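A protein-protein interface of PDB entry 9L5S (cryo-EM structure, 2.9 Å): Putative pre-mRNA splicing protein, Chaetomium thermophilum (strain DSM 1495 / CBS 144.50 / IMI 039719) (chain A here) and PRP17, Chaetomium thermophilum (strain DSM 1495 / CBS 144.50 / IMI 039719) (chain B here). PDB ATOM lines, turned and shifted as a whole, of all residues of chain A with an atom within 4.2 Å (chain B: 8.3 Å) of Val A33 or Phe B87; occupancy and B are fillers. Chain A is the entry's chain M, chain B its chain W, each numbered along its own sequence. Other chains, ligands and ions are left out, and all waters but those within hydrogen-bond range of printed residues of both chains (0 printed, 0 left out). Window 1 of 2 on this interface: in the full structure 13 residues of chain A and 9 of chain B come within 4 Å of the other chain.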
ATOM      1  N   PRO A  28     -30.817  10.286  38.934  1.00  0.00           N
ATOM      2  CA  PRO A  28     -31.847   9.248  38.808  1.00  0.00           C
ATOM      3  C   PRO A  28     -31.316   7.858  39.130  1.00  0.00           C
ATOM      4  O   PRO A  28     -30.120   7.582  39.020  1.00  0.00           O
ATOM      5  CB  PRO A  28     -32.270   9.349  37.339  1.00  0.00           C
ATOM      6  CG  PRO A  28     -32.002  10.755  36.978  1.00  0.00           C
ATOM      7  CD  PRO A  28     -30.754  11.128  37.726  1.00  0.00           C
ATOM      8  N   ASN A  30     -32.002   5.305  37.381  1.00  0.00           N
ATOM      9  CA  ASN A  30     -31.567   4.794  36.091  1.00  0.00           C
ATOM     10  C   ASN A  30     -30.092   5.126  35.879  1.00  0.00           C
ATOM     11  O   ASN A  30     -29.700   6.293  36.014  1.00  0.00           O
ATOM     12  CB  ASN A  30     -32.423   5.411  34.980  1.00  0.00           C
ATOM     13  CG  ASN A  30     -32.360   4.637  33.672  1.00  0.00           C
ATOM     14  OD1 ASN A  30     -31.340   4.046  33.323  1.00  0.00           O
ATOM     15  ND2 ASN A  30     -33.464   4.644  32.937  1.00  0.00           N
ATOM     16  N   PRO A  31     -29.248   4.142  35.552  1.00  0.00           N
ATOM     17  CA  PRO A  31     -27.838   4.442  35.251  1.00  0.00           C
ATOM     18  C   PRO A  31     -27.634   5.230  33.969  1.00  0.00           C
ATOM     19  O   PRO A  31     -26.497   5.625  33.684  1.00  0.00           O
ATOM     20  CB  PRO A  31     -27.196   3.053  35.142  1.00  0.00           C
ATOM     21  CG  PRO A  31     -28.119   2.139  35.855  1.00  0.00           C
ATOM     22  CD  PRO A  31     -29.490   2.696  35.674  1.00  0.00           C
ATOM     23  N   TYR A  32     -28.685   5.464  33.188  1.00  0.00           N
ATOM     24  CA  TYR A  32     -28.596   6.194  31.931  1.00  0.00           C
ATOM     25  C   TYR A  32     -29.430   7.456  32.090  1.00  0.00           C
ATOM     26  O   TYR A  32     -30.654   7.384  32.245  1.00  0.00           O
ATOM     27  CB  TYR A  32     -29.070   5.322  30.769  1.00  0.00           C
ATOM     28  CG  TYR A  32     -28.280   4.036  30.674  1.00  0.00           C
ATOM     29  CD1 TYR A  32     -27.091   3.977  29.960  1.00  0.00           C
ATOM     30  CD2 TYR A  32     -28.717   2.881  31.314  1.00  0.00           C
ATOM     31  CE1 TYR A  32     -26.362   2.805  29.885  1.00  0.00           C
ATOM     32  CE2 TYR A  32     -27.995   1.708  31.245  1.00  0.00           C
ATOM     33  CZ  TYR A  32     -26.819   1.675  30.530  1.00  0.00           C
ATOM     34  OH  TYR A  32     -26.099   0.506  30.455  1.00  0.00           O
ATOM     35  N   VAL A  33     -28.767   8.607  32.077  1.00  0.00           N
ATOM     36  CA  VAL A  33     -29.373   9.876  32.461  1.00  0.00           C
ATOM     37  C   VAL A  33     -29.559  10.721  31.210  1.00  0.00           C
ATOM     38  O   VAL A  33     -28.596  10.992  30.484  1.00  0.00           O
ATOM     39  CB  VAL A  33     -28.518  10.619  33.499  1.00  0.00           C
ATOM     40  CG1 VAL A  33     -29.311  11.753  34.130  1.00  0.00           C
ATOM     41  CG2 VAL A  33     -28.017   9.656  34.562  1.00  0.00           C
ATOM     42  N   LYS A  34     -30.797  11.131  30.958  1.00  0.00           N
ATOM     43  CA  LYS A  34     -31.099  12.110  29.925  1.00  0.00           C
ATOM     44  C   LYS A  34     -31.110  13.488  30.574  1.00  0.00           C
ATOM     45  O   LYS A  34     -31.924  13.754  31.465  1.00  0.00           O
ATOM     46  CB  LYS A  34     -32.438  11.801  29.263  1.00  0.00           C
ATOM     47  CG  LYS A  34     -32.462  10.476  28.526  1.00  0.00           C
ATOM     48  CD  LYS A  34     -33.683  10.366  27.635  1.00  0.00           C
ATOM     49  CE  LYS A  34     -34.952  10.268  28.460  1.00  0.00           C
ATOM     50  NZ  LYS A  34     -36.108   9.803  27.650  1.00  0.00           N
ATOM     51  N   MET A  35     -30.206  14.359  30.134  1.00  0.00           N
ATOM     52  CA  MET A  35     -29.939  15.611  30.825  1.00  0.00           C
ATOM     53  C   MET A  35     -30.033  16.782  29.856  1.00  0.00           C
ATOM     54  O   MET A  35     -29.501  16.725  28.744  1.00  0.00           O
ATOM     55  CB  MET A  35     -28.553  15.570  31.482  1.00  0.00           C
ATOM     56  CG  MET A  35     -28.211  16.769  32.342  1.00  0.00           C
ATOM     57  SD  MET A  35     -26.674  16.501  33.245  1.00  0.00           S
ATOM     58  CE  MET A  35     -27.249  15.497  34.610  1.00  0.00           C
ATOM     59  N   MET B  80     -17.558  10.594  25.742  1.00  0.00           N
ATOM     60  CA  MET B  80     -17.579   9.307  25.070  1.00  0.00           C
ATOM     61  C   MET B  80     -18.443   9.411  23.822  1.00  0.00           C
ATOM     62  O   MET B  80     -19.254  10.329  23.672  1.00  0.00           O
ATOM     63  CB  MET B  80     -18.095   8.207  26.005  1.00  0.00           C
ATOM     64  CG  MET B  80     -19.595   8.017  25.992  1.00  0.00           C
ATOM     65  SD  MET B  80     -20.106   6.902  27.304  1.00  0.00           S
ATOM     66  CE  MET B  80     -19.657   5.312  26.622  1.00  0.00           C
ATOM     67  N   ILE B  82     -20.938   7.010  21.512  1.00  0.00           N
ATOM     68  CA  ILE B  82     -21.697   5.800  21.237  1.00  0.00           C
ATOM     69  C   ILE B  82     -22.823   6.142  20.275  1.00  0.00           C
ATOM     70  O   ILE B  82     -23.165   7.307  20.063  1.00  0.00           O
ATOM     71  CB  ILE B  82     -22.269   5.139  22.508  1.00  0.00           C
ATOM     72  CG1 ILE B  82     -23.199   6.106  23.245  1.00  0.00           C
ATOM     73  CG2 ILE B  82     -21.163   4.597  23.389  1.00  0.00           C
ATOM     74  CD1 ILE B  82     -23.972   5.468  24.372  1.00  0.00           C
ATOM     75  N   SER B  83     -23.392   5.098  19.683  1.00  0.00           N
ATOM     76  CA  SER B  83     -24.559   5.267  18.840  1.00  0.00           C
ATOM     77  C   SER B  83     -25.762   5.691  19.678  1.00  0.00           C
ATOM     78  O   SER B  83     -25.845   5.418  20.879  1.00  0.00           O
ATOM     79  CB  SER B  83     -24.868   3.973  18.087  1.00  0.00           C
ATOM     80  OG  SER B  83     -25.352   2.976  18.968  1.00  0.00           O
ATOM     81  N   GLU B  84     -26.690   6.394  19.025  1.00  0.00           N
ATOM     82  CA  GLU B  84     -27.933   6.785  19.682  1.00  0.00           C
ATOM     83  C   GLU B  84     -28.754   5.561  20.070  1.00  0.00           C
ATOM     84  O   GLU B  84     -29.375   5.529  21.140  1.00  0.00           O
ATOM     85  CB  GLU B  84     -28.736   7.701  18.761  1.00  0.00           C
ATOM     86  CG  GLU B  84     -29.918   8.388  19.416  1.00  0.00           C
ATOM     87  CD  GLU B  84     -29.507   9.331  20.527  1.00  0.00           C
ATOM     88  OE1 GLU B  84     -28.472  10.014  20.378  1.00  0.00           O
ATOM     89  OE2 GLU B  84     -30.222   9.391  21.550  1.00  0.00           O
ATOM     90  N   ALA B  85     -28.757   4.541  19.204  1.00  0.00           N
ATOM     91  CA  ALA B  85     -29.539   3.335  19.447  1.00  0.00           C
ATOM     92  C   ALA B  85     -29.045   2.565  20.665  1.00  0.00           C
ATOM     93  O   ALA B  85     -29.857   1.966  21.374  1.00  0.00           O
ATOM     94  CB  ALA B  85     -29.512   2.438  18.210  1.00  0.00           C
ATOM     95  N   THR B  86     -27.734   2.576  20.927  1.00  0.00           N
ATOM     96  CA  THR B  86     -27.200   1.883  22.098  1.00  0.00           C
ATOM     97  C   THR B  86     -27.704   2.511  23.392  1.00  0.00           C
ATOM     98  O   THR B  86     -28.179   1.807  24.296  1.00  0.00           O
ATOM     99  CB  THR B  86     -25.670   1.896  22.060  1.00  0.00           C
ATOM    100  OG1 THR B  86     -25.213   1.287  20.847  1.00  0.00           O
ATOM    101  CG2 THR B  86     -25.096   1.140  23.245  1.00  0.00           C
ATOM    102  N   PHE B  87     -27.612   3.843  23.492  1.00  0.00           N
ATOM    103  CA  PHE B  87     -28.105   4.538  24.676  1.00  0.00           C
ATOM    104  C   PHE B  87     -29.608   4.367  24.827  1.00  0.00           C
ATOM    105  O   PHE B  87     -30.099   4.136  25.938  1.00  0.00           O
ATOM    106  CB  PHE B  87     -27.741   6.024  24.619  1.00  0.00           C
ATOM    107  CG  PHE B  87     -28.166   6.800  25.840  1.00  0.00           C
ATOM    108  CD1 PHE B  87     -27.365   6.821  26.970  1.00  0.00           C
ATOM    109  CD2 PHE B  87     -29.358   7.511  25.859  1.00  0.00           C
ATOM    110  CE1 PHE B  87     -27.746   7.527  28.095  1.00  0.00           C
ATOM    111  CE2 PHE B  87     -29.744   8.216  26.982  1.00  0.00           C
ATOM    112  CZ  PHE B  87     -28.936   8.225  28.100  1.00  0.00           C
ATOM    113  N   ARG B  88     -30.354   4.476  23.721  1.00  0.00           N
ATOM    114  CA  ARG B  88     -31.803   4.310  23.792  1.00  0.00           C
ATOM    115  C   ARG B  88     -32.187   2.901  24.224  1.00  0.00           C
ATOM    116  O   ARG B  88     -33.089   2.729  25.048  1.00  0.00           O
ATOM    117  CB  ARG B  88     -32.449   4.651  22.449  1.00  0.00           C
ATOM    118  CG  ARG B  88     -32.452   6.132  22.120  1.00  0.00           C
ATOM    119  CD  ARG B  88     -33.146   6.397  20.797  1.00  0.00           C
ATOM    120  NE  ARG B  88     -33.074   7.802  20.418  1.00  0.00           N
ATOM    121  CZ  ARG B  88     -34.019   8.696  20.674  1.00  0.00           C
ATOM    122  NH1 ARG B  88     -35.133   8.364  21.304  1.00  0.00           N
ATOM    123  NH2 ARG B  88     -33.841   9.955  20.287  1.00  0.00           N
ATOM    124  N   ALA B  89     -31.484   1.883  23.721  1.00  0.00           N
ATOM    125  CA  ALA B  89     -31.822   0.506  24.063  1.00  0.00           C
ATOM    126  C   ALA B  89     -31.474   0.184  25.511  1.00  0.00           C
ATOM    127  O   ALA B  89     -32.245  -0.493  26.199  1.00  0.00           O
ATOM    128  CB  ALA B  89     -31.118  -0.460  23.113  1.00  0.00           C
ATOM    129  N   LYS B  90     -30.333   0.674  26.005  1.00  0.00           N
ATOM    130  CA  LYS B  90     -29.978   0.405  27.398  1.00  0.00           C
ATOM    131  C   LYS B  90     -30.863   1.183  28.366  1.00  0.00           C
ATOM    132  O   LYS B  90     -31.294   0.641  29.397  1.00  0.00           O
ATOM    133  CB  LYS B  90     -28.503   0.718  27.634  1.00  0.00           C
ATOM    134  CG  LYS B  90     -27.572  -0.219  26.894  1.00  0.00           C
ATOM    135  CD  LYS B  90     -26.120   0.077  27.188  1.00  0.00           C
ATOM    136  CE  LYS B  90     -25.226  -0.830  26.372  1.00  0.00           C
ATOM    137  NZ  LYS B  90     -25.358  -2.246  26.815  1.00  0.00           N
ATOM    138  N   HIS B  91     -31.150   2.450  28.050  1.00  0.00           N
ATOM    139  CA  HIS B  91     -32.077   3.239  28.853  1.00  0.00           C
ATOM    140  C   HIS B  91     -33.469   2.626  28.840  1.00  0.00           C
ATOM    141  O   HIS B  91     -34.186   2.683  29.842  1.00  0.00           O
ATOM    142  CB  HIS B  91     -32.106   4.679  28.335  1.00  0.00           C
ATOM    143  CG  HIS B  91     -32.961   5.604  29.142  1.00  0.00           C
ATOM    144  ND1 HIS B  91     -34.338   5.618  29.058  1.00  0.00           N
ATOM    145  CD2 HIS B  91     -32.633   6.555  30.046  1.00  0.00           C
ATOM    146  CE1 HIS B  91     -34.818   6.534  29.879  1.00  0.00           C
ATOM    147  NE2 HIS B  91     -33.804   7.118  30.491  1.00  0.00           N
ATOM    148  N   ARG B  92     -33.872   2.044  27.710  1.00  0.00           N
ATOM    149  CA  ARG B  92     -35.160   1.369  27.630  1.00  0.00           C
ATOM    150  C   ARG B  92     -35.170   0.089  28.455  1.00  0.00           C
ATOM    151  O   ARG B  92     -36.165  -0.218  29.120  1.00  0.00           O
ATOM    152  CB  ARG B  92     -35.486   1.076  26.166  1.00  0.00           C
ATOM    153  CG  ARG B  92     -36.647   0.128  25.939  1.00  0.00           C
ATOM    154  CD  ARG B  92     -37.957   0.792  26.326  1.00  0.00           C
ATOM    155  NE  ARG B  92     -37.961   2.218  26.024  1.00  0.00           N
ATOM    156  CZ  ARG B  92     -38.170   2.739  24.823  1.00  0.00           C
ATOM    157  NH1 ARG B  92     -38.402   1.974  23.769  1.00  0.00           N
ATOM    158  NH2 ARG B  92     -38.144   4.060  24.675  1.00  0.00           N
ATOM    159  N   ALA B  93     -34.073  -0.671  28.417  1.00  0.00           N
ATOM    160  CA  ALA B  93     -33.986  -1.905  29.189  1.00  0.00           C
ATOM    161  C   ALA B  93     -34.068  -1.627  30.683  1.00  0.00           C
ATOM    162  O   ALA B  93     -34.718  -2.372  31.425  1.00  0.00           O
ATOM    163  CB  ALA B  93     -32.695  -2.648  28.851  1.00  0.00           C
ATOM    164  N   VAL B  94     -33.412  -0.561  31.146  1.00  0.00           N
ATOM    165  CA  VAL B  94     -33.533  -0.198  32.556  1.00  0.00           C
ATOM    166  C   VAL B  94     -34.917   0.377  32.853  1.00  0.00           C
ATOM    167  O   VAL B  94     -35.563  -0.003  33.838  1.00  0.00           O
ATOM    168  CB  VAL B  94     -32.417   0.780  32.961  1.00  0.00           C
ATOM    169  CG1 VAL B  94     -32.579   1.178  34.417  1.00  0.00           C
ATOM    170  CG2 VAL B  94     -31.054   0.157  32.725  1.00  0.00           C
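The side-chain amide nitrogen (ND2) of Asn A30 is in hydrogen-bond range of a ring nitrogen (NE2) of His B91 (3.5 Å).
The side-chain amide oxygen of Asn A30 lies within hydrogen-bond range of the backbone NH of Tyr A32.
Among the printed residues, merely in contact across the chains: Asn A30 with Val B94 (3.3 Å), Pro A31 with Val B94 (3.7 Å), Tyr A32 with Phe B87 (3.7 Å), Tyr A32 with Lys B90 (3.3 Å), Tyr A32 with His B91 (3.1 Å), Tyr A32 with Val B94 (3.7 Å), Val A33 with Phe B87 (3.7 Å), Lys A34 with Phe B87 (3.9 Å) and Lys A34 with His B91 (3.9 Å).
Printed residues of chain B within 4 Å of Asn A30: His B91 (3.5 Å) and Val B94 (3.3 Å).
Printed residues of chain B within 4 Å of Pro A31: Val B94 (3.7 Å).
Val A33 touches just one residue of chain B: Phe B87 (3.7 Å).
Ile B82 touches none of the printed residues of chain A.
Phe B87 touches three residues of chain A.
Of the printed residues of chain A, Lys B90 touches Tyr A32.
Of the printed residues of chain A, Val B94 touches Asn A30, Pro A31 and Tyr A32.
The nearest residue of chain B that does not touch Val A33 is His B91 (4.8 Å).
The nearest printed residue of chain B that does not touch Tyr A32 is Thr B86 (6.0 Å).
Of the 14 printed residues of chain B, 4 touch a printed residue of chain A.
Of the 7 printed residues of chain A, 5 touch a printed residue of chain B.
Among the printed residues, 10 pairs touch across the chains.
Among the printed residues, no Asp or Glu carboxylate lies within 4 Å of a Lys or Arg side-chain nitrogen of the other chain.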
